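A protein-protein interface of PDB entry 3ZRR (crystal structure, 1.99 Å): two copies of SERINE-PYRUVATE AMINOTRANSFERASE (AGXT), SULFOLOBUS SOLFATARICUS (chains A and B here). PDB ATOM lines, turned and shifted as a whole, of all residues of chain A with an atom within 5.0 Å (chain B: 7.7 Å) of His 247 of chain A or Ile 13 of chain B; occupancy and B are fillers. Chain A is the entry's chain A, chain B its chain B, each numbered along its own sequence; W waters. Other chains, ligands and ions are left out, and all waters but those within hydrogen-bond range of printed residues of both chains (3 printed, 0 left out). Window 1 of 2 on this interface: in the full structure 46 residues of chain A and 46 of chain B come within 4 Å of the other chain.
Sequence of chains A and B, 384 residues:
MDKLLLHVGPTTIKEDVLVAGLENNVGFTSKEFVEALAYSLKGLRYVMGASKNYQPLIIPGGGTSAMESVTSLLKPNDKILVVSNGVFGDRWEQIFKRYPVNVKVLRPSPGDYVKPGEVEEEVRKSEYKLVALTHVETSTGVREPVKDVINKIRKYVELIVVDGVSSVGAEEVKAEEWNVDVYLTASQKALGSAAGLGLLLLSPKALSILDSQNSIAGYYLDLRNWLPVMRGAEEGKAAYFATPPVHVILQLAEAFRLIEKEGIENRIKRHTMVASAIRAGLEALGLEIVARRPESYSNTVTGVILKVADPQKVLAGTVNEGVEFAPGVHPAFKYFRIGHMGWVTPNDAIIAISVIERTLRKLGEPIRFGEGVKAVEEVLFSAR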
ATOM      1  N   GLY A  21     -38.592  -4.821  -0.631  1.00  0.00           N
ATOM      2  CA  GLY A  21     -37.360  -5.264   0.022  1.00  0.00           C
ATOM      3  C   GLY A  21     -36.061  -4.886  -0.684  1.00  0.00           C
ATOM      4  O   GLY A  21     -34.984  -5.202  -0.190  1.00  0.00           O
ATOM      5  N   GLU A  23     -34.104  -2.276  -0.840  1.00  0.00           N
ATOM      6  CA  GLU A  23     -33.389  -1.104  -0.349  1.00  0.00           C
ATOM      7  C   GLU A  23     -32.055  -1.600   0.197  1.00  0.00           C
ATOM      8  O   GLU A  23     -32.024  -2.289   1.219  1.00  0.00           O
ATOM      9  CB  GLU A  23     -34.195  -0.422   0.755  1.00  0.00           C
ATOM     10  CG  GLU A  23     -35.634  -0.080   0.382  1.00  0.00           C
ATOM     11  CD  GLU A  23     -35.753   1.248  -0.361  1.00  0.00           C
ATOM     12  OE1 GLU A  23     -34.716   1.897  -0.634  1.00  0.00           O
ATOM     13  OE2 GLU A  23     -36.891   1.664  -0.672  1.00  0.00           O
ATOM     14  N   ASN A  24     -30.955  -1.268  -0.477  1.00  0.00           N
ATOM     15  CA  ASN A  24     -29.660  -1.934  -0.201  1.00  0.00           C
ATOM     16  C   ASN A  24     -28.731  -1.301   0.853  1.00  0.00           C
ATOM     17  O   ASN A  24     -27.580  -1.748   1.030  1.00  0.00           O
ATOM     18  CB  ASN A  24     -28.900  -2.238  -1.504  1.00  0.00           C
ATOM     19  CG  ASN A  24     -28.447  -0.989  -2.242  1.00  0.00           C
ATOM     20  OD1 ASN A  24     -28.785   0.144  -1.878  1.00  0.00           O
ATOM     21  ND2 ASN A  24     -27.690  -1.197  -3.310  1.00  0.00           N
ATOM     22  N   VAL A  26     -30.051  -0.441   4.201  1.00  0.00           N
ATOM     23  CA  VAL A  26     -30.947  -0.409   5.358  1.00  0.00           C
ATOM     24  C   VAL A  26     -30.520  -1.439   6.414  1.00  0.00           C
ATOM     25  O   VAL A  26     -30.219  -2.597   6.083  1.00  0.00           O
ATOM     26  CB  VAL A  26     -32.437  -0.635   4.895  1.00  0.00           C
ATOM     27  CG1 VAL A  26     -33.396  -0.871   6.076  1.00  0.00           C
ATOM     28  CG2 VAL A  26     -32.914   0.563   4.078  1.00  0.00           C
ATOM     29  N   PRO A 245     -34.856 -10.086  10.418  1.00  0.00           N
ATOM     30  CA  PRO A 245     -34.777 -10.138   8.966  1.00  0.00           C
ATOM     31  C   PRO A 245     -35.269  -8.795   8.387  1.00  0.00           C
ATOM     32  O   PRO A 245     -36.441  -8.649   8.014  1.00  0.00           O
ATOM     33  CB  PRO A 245     -35.678 -11.326   8.609  1.00  0.00           C
ATOM     34  CG  PRO A 245     -35.938 -12.047   9.941  1.00  0.00           C
ATOM     35  CD  PRO A 245     -35.934 -10.941  10.927  1.00  0.00           C
ATOM     36  N   VAL A 246     -34.346  -7.830   8.337  1.00  0.00           N
ATOM     37  CA  VAL A 246     -34.627  -6.420   8.025  1.00  0.00           C
ATOM     38  C   VAL A 246     -35.489  -6.257   6.763  1.00  0.00           C
ATOM     39  O   VAL A 246     -36.519  -5.588   6.791  1.00  0.00           O
ATOM     40  CB  VAL A 246     -33.288  -5.612   7.894  1.00  0.00           C
ATOM     41  CG1 VAL A 246     -33.545  -4.179   7.477  1.00  0.00           C
ATOM     42  CG2 VAL A 246     -32.511  -5.621   9.239  1.00  0.00           C
ATOM     43  N   HIS A 247     -35.073  -6.873   5.663  1.00  0.00           N
ATOM     44  CA  HIS A 247     -35.769  -6.684   4.392  1.00  0.00           C
ATOM     45  C   HIS A 247     -37.085  -7.439   4.304  1.00  0.00           C
ATOM     46  O   HIS A 247     -37.991  -7.015   3.586  1.00  0.00           O
ATOM     47  CB  HIS A 247     -34.864  -7.064   3.236  1.00  0.00           C
ATOM     48  CG  HIS A 247     -33.663  -6.186   3.125  1.00  0.00           C
ATOM     49  ND1 HIS A 247     -32.499  -6.420   3.831  1.00  0.00           N
ATOM     50  CD2 HIS A 247     -33.450  -5.057   2.409  1.00  0.00           C
ATOM     51  CE1 HIS A 247     -31.616  -5.478   3.542  1.00  0.00           C
ATOM     52  NE2 HIS A 247     -32.165  -4.644   2.675  1.00  0.00           N
ATOM     53  N   VAL A 248     -37.199  -8.538   5.039  1.00  0.00           N
ATOM     54  CA  VAL A 248     -38.471  -9.285   5.117  1.00  0.00           C
ATOM     55  C   VAL A 248     -39.502  -8.411   5.826  1.00  0.00           C
ATOM     56  O   VAL A 248     -40.683  -8.423   5.495  1.00  0.00           O
ATOM     57  CB  VAL A 248     -38.288 -10.647   5.887  1.00  0.00           C
ATOM     58  CG1 VAL A 248     -39.600 -11.420   5.943  1.00  0.00           C
ATOM     59  CG2 VAL A 248     -37.243 -11.517   5.207  1.00  0.00           C
ATOM     60  N   ILE A 249     -39.039  -7.631   6.802  1.00  0.00           N
ATOM     61  CA  ILE A 249     -39.933  -6.730   7.530  1.00  0.00           C
ATOM     62  C   ILE A 249     -40.326  -5.516   6.660  1.00  0.00           C
ATOM     63  O   ILE A 249     -41.440  -5.011   6.758  1.00  0.00           O
ATOM     64  CB  ILE A 249     -39.325  -6.293   8.862  1.00  0.00           C
ATOM     65  CG1 ILE A 249     -39.269  -7.496   9.818  1.00  0.00           C
ATOM     66  CG2 ILE A 249     -40.169  -5.172   9.504  1.00  0.00           C
ATOM     67  CD1 ILE A 249     -38.386  -7.299  11.060  1.00  0.00           C
ATOM     68  N   LEU A 250     -39.430  -5.072   5.788  1.00  0.00           N
ATOM     69  CA  LEU A 250     -39.790  -4.021   4.822  1.00  0.00           C
ATOM     70  C   LEU A 250     -40.915  -4.526   3.924  1.00  0.00           C
ATOM     71  O   LEU A 250     -41.880  -3.806   3.654  1.00  0.00           O
ATOM     72  CB  LEU A 250     -38.575  -3.598   3.961  1.00  0.00           C
ATOM     73  CG  LEU A 250     -37.437  -2.884   4.701  1.00  0.00           C
ATOM     74  CD1 LEU A 250     -36.302  -2.493   3.791  1.00  0.00           C
ATOM     75  CD2 LEU A 250     -37.956  -1.666   5.417  1.00  0.00           C
ATOM     76  N   GLN A 251     -40.779  -5.772   3.472  1.00  0.00           N
ATOM     77  CA  GLN A 251     -41.776  -6.432   2.646  1.00  0.00           C
ATOM     78  C   GLN A 251     -43.106  -6.587   3.376  1.00  0.00           C
ATOM     79  O   GLN A 251     -44.169  -6.324   2.799  1.00  0.00           O
ATOM     80  CB  GLN A 251     -41.231  -7.774   2.138  1.00  0.00           C
ATOM     81  CG  GLN A 251     -40.036  -7.576   1.206  1.00  0.00           C
ATOM     82  CD  GLN A 251     -39.276  -8.863   0.853  1.00  0.00           C
ATOM     83  OE1 GLN A 251     -39.069  -9.738   1.683  1.00  0.00           O
ATOM     84  NE2 GLN A 251     -38.823  -8.946  -0.394  1.00  0.00           N
ATOM     85  N   PRO B  10     -25.031  -0.093   8.492  1.00  0.00           N
ATOM     86  CA  PRO B  10     -25.444  -1.328   7.811  1.00  0.00           C
ATOM     87  C   PRO B  10     -24.451  -1.775   6.733  1.00  0.00           C
ATOM     88  O   PRO B  10     -23.975  -0.942   5.950  1.00  0.00           O
ATOM     89  CB  PRO B  10     -26.783  -0.943   7.175  1.00  0.00           C
ATOM     90  CG  PRO B  10     -26.695   0.536   6.949  1.00  0.00           C
ATOM     91  CD  PRO B  10     -25.677   1.102   7.909  1.00  0.00           C
ATOM     92  N   THR B  11     -24.137  -3.071   6.704  1.00  0.00           N
ATOM     93  CA  THR B  11     -23.288  -3.634   5.647  1.00  0.00           C
ATOM     94  C   THR B  11     -24.022  -3.446   4.305  1.00  0.00           C
ATOM     95  O   THR B  11     -25.171  -3.883   4.157  1.00  0.00           O
ATOM     96  CB  THR B  11     -22.916  -5.137   5.923  1.00  0.00           C
ATOM     97  OG1 THR B  11     -22.299  -5.256   7.211  1.00  0.00           O
ATOM     98  CG2 THR B  11     -21.950  -5.690   4.872  1.00  0.00           C
ATOM     99  N   THR B  12     -23.371  -2.752   3.366  1.00  0.00           N
ATOM    100  CA  THR B  12     -23.914  -2.516   2.017  1.00  0.00           C
ATOM    101  C   THR B  12     -24.050  -3.838   1.261  1.00  0.00           C
ATOM    102  O   THR B  12     -23.126  -4.662   1.247  1.00  0.00           O
ATOM    103  CB  THR B  12     -23.021  -1.562   1.176  1.00  0.00           C
ATOM    104  OG1 THR B  12     -22.534  -0.492   1.999  1.00  0.00           O
ATOM    105  CG2 THR B  12     -23.791  -1.002  -0.037  1.00  0.00           C
ATOM    106  N   ILE B  13     -25.215  -4.038   0.652  1.00  0.00           N
ATOM    107  CA  ILE B  13     -25.493  -5.267  -0.080  1.00  0.00           C
ATOM    108  C   ILE B  13     -25.465  -4.972  -1.580  1.00  0.00           C
ATOM    109  O   ILE B  13     -26.126  -4.049  -2.041  1.00  0.00           O
ATOM    110  CB  ILE B  13     -26.872  -5.882   0.333  1.00  0.00           C
ATOM    111  CG1 ILE B  13     -26.993  -5.996   1.871  1.00  0.00           C
ATOM    112  CG2 ILE B  13     -27.085  -7.220  -0.365  1.00  0.00           C
ATOM    113  CD1 ILE B  13     -28.371  -6.368   2.394  1.00  0.00           C
ATOM    114  N   LYS B  14     -24.696  -5.744  -2.337  1.00  0.00           N
ATOM    115  CA  LYS B  14     -24.731  -5.629  -3.791  1.00  0.00           C
ATOM    116  C   LYS B  14     -26.169  -5.801  -4.231  1.00  0.00           C
ATOM    117  O   LYS B  14     -26.881  -6.668  -3.714  1.00  0.00           O
ATOM    118  CB  LYS B  14     -23.856  -6.684  -4.463  1.00  0.00           C
ATOM    119  CG  LYS B  14     -22.426  -6.263  -4.611  1.00  0.00           C
ATOM    120  CD  LYS B  14     -21.673  -7.160  -5.552  1.00  0.00           C
ATOM    121  CE  LYS B  14     -20.477  -6.401  -6.080  1.00  0.00           C
ATOM    122  NZ  LYS B  14     -19.807  -7.089  -7.216  1.00  0.00           N
ATOM    123  N   GLU B  15     -26.593  -4.953  -5.166  1.00  0.00           N
ATOM    124  CA  GLU B  15     -27.957  -5.007  -5.675  1.00  0.00           C
ATOM    125  C   GLU B  15     -28.289  -6.364  -6.266  1.00  0.00           C
ATOM    126  O   GLU B  15     -29.391  -6.860  -6.046  1.00  0.00           O
ATOM    127  CB  GLU B  15     -28.220  -3.914  -6.710  1.00  0.00           C
ATOM    128  CG  GLU B  15     -29.704  -3.567  -6.818  1.00  0.00           C
ATOM    129  CD  GLU B  15     -30.272  -3.007  -5.510  1.00  0.00           C
ATOM    130  OE1 GLU B  15     -29.615  -2.141  -4.892  1.00  0.00           O
ATOM    131  OE2 GLU B  15     -31.372  -3.437  -5.102  1.00  0.00           O
ATOM    132  N   ASP B  16     -27.343  -6.963  -7.001  1.00  0.00           N
ATOM    133  CA  ASP B  16     -27.506  -8.323  -7.535  1.00  0.00           C
ATOM    134  C   ASP B  16     -27.932  -9.313  -6.464  1.00  0.00           C
ATOM    135  O   ASP B  16     -28.734 -10.187  -6.721  1.00  0.00           O
ATOM    136  CB  ASP B  16     -26.208  -8.837  -8.167  1.00  0.00           C
ATOM    137  CG  ASP B  16     -25.893  -8.163  -9.489  1.00  0.00           C
ATOM    138  OD1 ASP B  16     -26.644  -8.356 -10.476  1.00  0.00           O
ATOM    139  OD2 ASP B  16     -24.873  -7.447  -9.554  1.00  0.00           O
ATOM    140  N   VAL B  17     -27.368  -9.179  -5.266  1.00  0.00           N
ATOM    141  CA  VAL B  17     -27.745 -10.057  -4.151  1.00  0.00           C
ATOM    142  C   VAL B  17     -29.242  -9.881  -3.805  1.00  0.00           C
ATOM    143  O   VAL B  17     -30.007 -10.863  -3.758  1.00  0.00           O
ATOM    144  CB  VAL B  17     -26.828  -9.833  -2.929  1.00  0.00           C
ATOM    145  CG1 VAL B  17     -27.300 -10.662  -1.765  1.00  0.00           C
ATOM    146  CG2 VAL B  17     -25.380 -10.213  -3.263  1.00  0.00           C
ATOM    147  N   LEU B  18     -29.652  -8.631  -3.593  1.00  0.00           N
ATOM    148  CA  LEU B  18     -31.040  -8.338  -3.255  1.00  0.00           C
ATOM    149  C   LEU B  18     -32.016  -8.766  -4.332  1.00  0.00           C
ATOM    150  O   LEU B  18     -33.029  -9.421  -4.049  1.00  0.00           O
ATOM    151  CB  LEU B  18     -31.224  -6.853  -2.930  1.00  0.00           C
ATOM    152  CG  LEU B  18     -30.596  -6.381  -1.623  1.00  0.00           C
ATOM    153  CD1 LEU B  18     -31.110  -5.019  -1.320  1.00  0.00           C
ATOM    154  CD2 LEU B  18     -30.920  -7.321  -0.462  1.00  0.00           C
ATOM    155  N   VAL B  19     -31.684  -8.414  -5.569  1.00  0.00           N
ATOM    156  CA  VAL B  19     -32.527  -8.667  -6.720  1.00  0.00           C
ATOM    157  C   VAL B  19     -32.768 -10.149  -6.932  1.00  0.00           C
ATOM    158  O   VAL B  19     -33.823 -10.524  -7.440  1.00  0.00           O
ATOM    159  CB  VAL B  19     -31.919  -7.986  -7.982  1.00  0.00           C
ATOM    160  CG1 VAL B  19     -32.444  -8.588  -9.274  1.00  0.00           C
ATOM    161  CG2 VAL B  19     -32.172  -6.484  -7.914  1.00  0.00           C
ATOM    162  N   SER B 187     -25.880 -14.261   7.982  1.00  0.00           N
ATOM    163  CA  SER B 187     -25.885 -13.922   6.568  1.00  0.00           C
ATOM    164  C   SER B 187     -25.507 -12.451   6.285  1.00  0.00           C
ATOM    165  O   SER B 187     -25.070 -12.137   5.183  1.00  0.00           O
ATOM    166  CB  SER B 187     -27.244 -14.272   5.929  1.00  0.00           C
ATOM    167  OG  SER B 187     -28.321 -13.690   6.659  1.00  0.00           O
ATOM    168  N   GLN B 188     -25.656 -11.571   7.275  1.00  0.00           N
ATOM    169  CA  GLN B 188     -25.645 -10.129   7.004  1.00  0.00           C
ATOM    170  C   GLN B 188     -24.328  -9.395   7.292  1.00  0.00           C
ATOM    171  O   GLN B 188     -24.280  -8.181   7.171  1.00  0.00           O
ATOM    172  CB  GLN B 188     -26.801  -9.410   7.728  1.00  0.00           C
ATOM    173  CG  GLN B 188     -26.579  -9.117   9.247  1.00  0.00           C
ATOM    174  CD  GLN B 188     -26.771 -10.337  10.133  1.00  0.00           C
ATOM    175  OE1 GLN B 188     -27.157 -11.412   9.674  1.00  0.00           O
ATOM    176  NE2 GLN B 188     -26.476 -10.178  11.415  1.00  0.00           N
ATOM    177  N   LYS B 189     -23.271 -10.104   7.677  1.00  0.00           N
ATOM    178  CA  LYS B 189     -22.036  -9.396   8.056  1.00  0.00           C
ATOM    179  C   LYS B 189     -20.978  -9.523   6.949  1.00  0.00           C
ATOM    180  O   LYS B 189     -21.203  -9.047   5.819  1.00  0.00           O
ATOM    181  CB  LYS B 189     -21.556  -9.825   9.455  1.00  0.00           C
ATOM    182  CG  LYS B 189     -22.426  -9.270  10.605  1.00  0.00           C
ATOM    183  CD  LYS B 189     -22.306  -7.749  10.724  1.00  0.00           C
ATOM    184  CE  LYS B 189     -23.414  -7.138  11.590  1.00  0.00           C
ATOM    185  NZ  LYS B 189     -23.443  -5.618  11.553  1.00  0.00           N
ATOM    186  N   LEU B 191     -20.239 -11.853   5.056  1.00  0.00           N
ATOM    187  CA  LEU B 191     -20.759 -12.480   3.841  1.00  0.00           C
ATOM    188  C   LEU B 191     -21.525 -11.475   2.949  1.00  0.00           C
ATOM    189  O   LEU B 191     -21.693 -11.714   1.744  1.00  0.00           O
ATOM    190  CB  LEU B 191     -21.653 -13.682   4.173  1.00  0.00           C
ATOM    191  CG  LEU B 191     -20.990 -14.892   4.845  1.00  0.00           C
ATOM    192  CD1 LEU B 191     -22.042 -15.952   5.183  1.00  0.00           C
ATOM    193  CD2 LEU B 191     -19.882 -15.490   3.929  1.00  0.00           C
ATOM    194  N   GLY B 192     -22.011 -10.384   3.541  1.00  0.00           N
ATOM    195  CA  GLY B 192     -22.656  -9.302   2.776  1.00  0.00           C
ATOM    196  C   GLY B 192     -24.003  -9.602   2.120  1.00  0.00           C
ATOM    197  O   GLY B 192     -24.367  -8.981   1.116  1.00  0.00           O
ATOM    198  N   SER B 193     -24.762 -10.538   2.681  1.00  0.00           N
ATOM    199  CA  SER B 193     -26.083 -10.856   2.141  1.00  0.00           C
ATOM    200  C   SER B 193     -27.195 -10.240   3.010  1.00  0.00           C
ATOM    201  O   SER B 193     -26.912  -9.530   3.982  1.00  0.00           O
ATOM    202  CB  SER B 193     -26.260 -12.362   2.016  1.00  0.00           C
ATOM    203  OG  SER B 193     -27.386 -12.679   1.210  1.00  0.00           O
ATOM    204  N   ALA B 194     -28.446 -10.533   2.689  1.00  0.00           N
ATOM    205  CA  ALA B 194     -29.567 -10.004   3.498  1.00  0.00           C
ATOM    206  C   ALA B 194     -29.719 -10.749   4.826  1.00  0.00           C
ATOM    207  O   ALA B 194     -29.463 -11.959   4.915  1.00  0.00           O
ATOM    208  CB  ALA B 194     -30.874 -10.094   2.690  1.00  0.00           C
ATOM    209  N   ALA B 195     -30.159 -10.018   5.855  1.00  0.00           N
ATOM    210  CA  ALA B 195     -30.342 -10.554   7.214  1.00  0.00           C
ATOM    211  C   ALA B 195     -31.465 -11.587   7.259  1.00  0.00           C
ATOM    212  O   ALA B 195     -32.402 -11.537   6.442  1.00  0.00           O
ATOM    213  CB  ALA B 195     -30.643  -9.421   8.185  1.00  0.00           C
ATOM    214  N   GLY B 196     -31.368 -12.524   8.207  1.00  0.00           N
ATOM    215  CA  GLY B 196     -32.447 -13.474   8.472  1.00  0.00           C
ATOM    216  C   GLY B 196     -31.999 -14.909   8.725  1.00  0.00           C
ATOM    217  O   GLY B 196     -32.822 -15.754   9.040  1.00  0.00           O
ATOM    218  N   VAL B 248     -34.659 -14.977   1.422  1.00  0.00           N
ATOM    219  CA  VAL B 248     -33.364 -14.595   2.032  1.00  0.00           C
ATOM    220  C   VAL B 248     -32.323 -15.643   1.624  1.00  0.00           C
ATOM    221  O   VAL B 248     -31.159 -15.324   1.391  1.00  0.00           O
ATOM    222  CB  VAL B 248     -33.464 -14.501   3.586  1.00  0.00           C
ATOM    223  CG1 VAL B 248     -32.120 -14.108   4.199  1.00  0.00           C
ATOM    224  CG2 VAL B 248     -34.561 -13.518   4.014  1.00  0.00           C
ATOM    225  N   GLN B 251     -31.272 -15.038  -1.932  1.00  0.00           N
ATOM    226  CA  GLN B 251     -30.290 -13.953  -1.873  1.00  0.00           C
ATOM    227  C   GLN B 251     -28.914 -14.455  -1.433  1.00  0.00           C
ATOM    228  O   GLN B 251     -27.901 -14.086  -2.024  1.00  0.00           O
ATOM    229  CB  GLN B 251     -30.811 -12.823  -0.975  1.00  0.00           C
ATOM    230  CG  GLN B 251     -32.074 -12.183  -1.575  1.00  0.00           C
ATOM    231  CD  GLN B 251     -32.796 -11.219  -0.645  1.00  0.00           C
ATOM    232  OE1 GLN B 251     -32.927 -11.463   0.558  1.00  0.00           O
ATOM    233  NE2 GLN B 251     -33.298 -10.111  -1.213  1.00  0.00           N
ATOM    234  N   ALA B 255     -25.148 -14.309  -3.121  1.00  0.00           N
ATOM    235  CA  ALA B 255     -23.936 -13.848  -2.422  1.00  0.00           C
ATOM    236  C   ALA B 255     -22.820 -14.891  -2.535  1.00  0.00           C
ATOM    237  O   ALA B 255     -21.681 -14.539  -2.842  1.00  0.00           O
ATOM    238  CB  ALA B 255     -24.224 -13.496  -0.962  1.00  0.00           C
ATOM    239  N   TRP B 343     -18.426  -6.466   0.787  1.00  0.00           N
ATOM    240  CA  TRP B 343     -18.091  -6.085  -0.580  1.00  0.00           C
ATOM    241  C   TRP B 343     -17.176  -4.862  -0.589  1.00  0.00           C
ATOM    242  O   TRP B 343     -16.941  -4.279  -1.641  1.00  0.00           O
ATOM    243  CB  TRP B 343     -19.368  -5.836  -1.416  1.00  0.00           C
ATOM    244  CG  TRP B 343     -20.407  -6.924  -1.237  1.00  0.00           C
ATOM    245  CD1 TRP B 343     -21.578  -6.828  -0.529  1.00  0.00           C
ATOM    246  CD2 TRP B 343     -20.355  -8.277  -1.744  1.00  0.00           C
ATOM    247  NE1 TRP B 343     -22.271  -8.024  -0.583  1.00  0.00           N
ATOM    248  CE2 TRP B 343     -21.543  -8.933  -1.308  1.00  0.00           C
ATOM    249  CE3 TRP B 343     -19.435  -8.988  -2.529  1.00  0.00           C
ATOM    250  CZ2 TRP B 343     -21.826 -10.276  -1.619  1.00  0.00           C
ATOM    251  CZ3 TRP B 343     -19.710 -10.313  -2.849  1.00  0.00           C
ATOM    252  CH2 TRP B 343     -20.898 -10.951  -2.383  1.00  0.00           C
HETATM  253  O   HOH W   1     -33.904  -9.585   5.107  1.00  0.00           O
HETATM  254  O   HOH W   2     -35.200  -8.233   0.055  1.00  0.00           O
HETATM  255  O   HOH W   3     -30.077  -7.130   5.826  1.00  0.00           O
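The backbone carbonyl oxygen (O) of Leu 18 of chain B lies within hydrogen-bond range of the side-chain amide nitrogen (NE2) of Gln 251 of chain B. The backbone carbonyl oxygen (O) of Glu 23 of chain A sits at hydrogen-bond distance from a ring nitrogen (NE2) of His 247 of chain A (2.8 Å). The side-chain amide oxygen (OE1) of Gln 251 of chain A lies close to the backbone carbonyl oxygen (O) of His 247 of chain A, at 3.5 Å.
Printed residues of chain B that touch a printed residue of chain A: Pro 10, Thr 12, Ile 13, Glu 15, Leu 18, Ala 195, Gly 196 and Val 248. Along chain B the printed residues that touch a printed residue of chain A span positions 10 to 248. Among the printed residues, 10 pairs touch across the chains.
Of chain B, only Ile 13 (3.6 Å) comes within 4 Å of His 247 of chain A. Printed residues of chain A within 4 Å of Thr 12 of chain B: Asn 24 (3.9 Å). Of the printed residues of chain A, Val 248 of chain B touches Val 248. The nearest printed residue of chain A that does not touch Ile 13 of chain B is Val 26 of chain A (5.6 Å). The nearest printed residue of chain A that does not touch Glu 15 of chain B is Glu 23 of chain A (5.2 Å).
The side-chain carboxylate (OE1) of Glu 15 of chain B is in hydrogen-bond range of the side-chain amide nitrogen (ND2) of Asn 24 of chain A (2.7 Å). The backbone carbonyl oxygen (O) of Asn 24 of chain A sits at hydrogen-bond distance from the backbone NH (N) of Ile 13 of chain B (3.3 Å).
Val 248 of chain A touches its own counterpart, Val 248 of chain B.
Among the printed residues, merely in contact across the chains: Val 248 of chain A with Val 248 of chain B, His 247 of chain A with Ile 13 of chain B, Asn 24 of chain A with Leu 18 of chain B, Pro 245 of chain A with Ala 195 of chain B, Glu 23 of chain A with Leu 18 of chain B, Val 26 of chain A with Pro 10 of chain B, Asn 24 of chain A with Thr 12 of chain B and Pro 245 of chain A with Gly 196 of chain B.
Water W1 lies within hydrogen-bond range of O of Ala 195 of chain B (2.8 Å), N of His 247 of chain A (3.0 Å) and N of Val 248 of chain A (3.5 Å). Water W3 bridges the backbone NH (N) of Ala 195 of chain B (2.9 Å) and a ring nitrogen (ND1) of His 247 of chain A (3.2 Å). Water W2 bridges the side-chain amide nitrogen of Gln 251 of chain B and the backbone carbonyl oxygen of Gly 21 of chain A.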
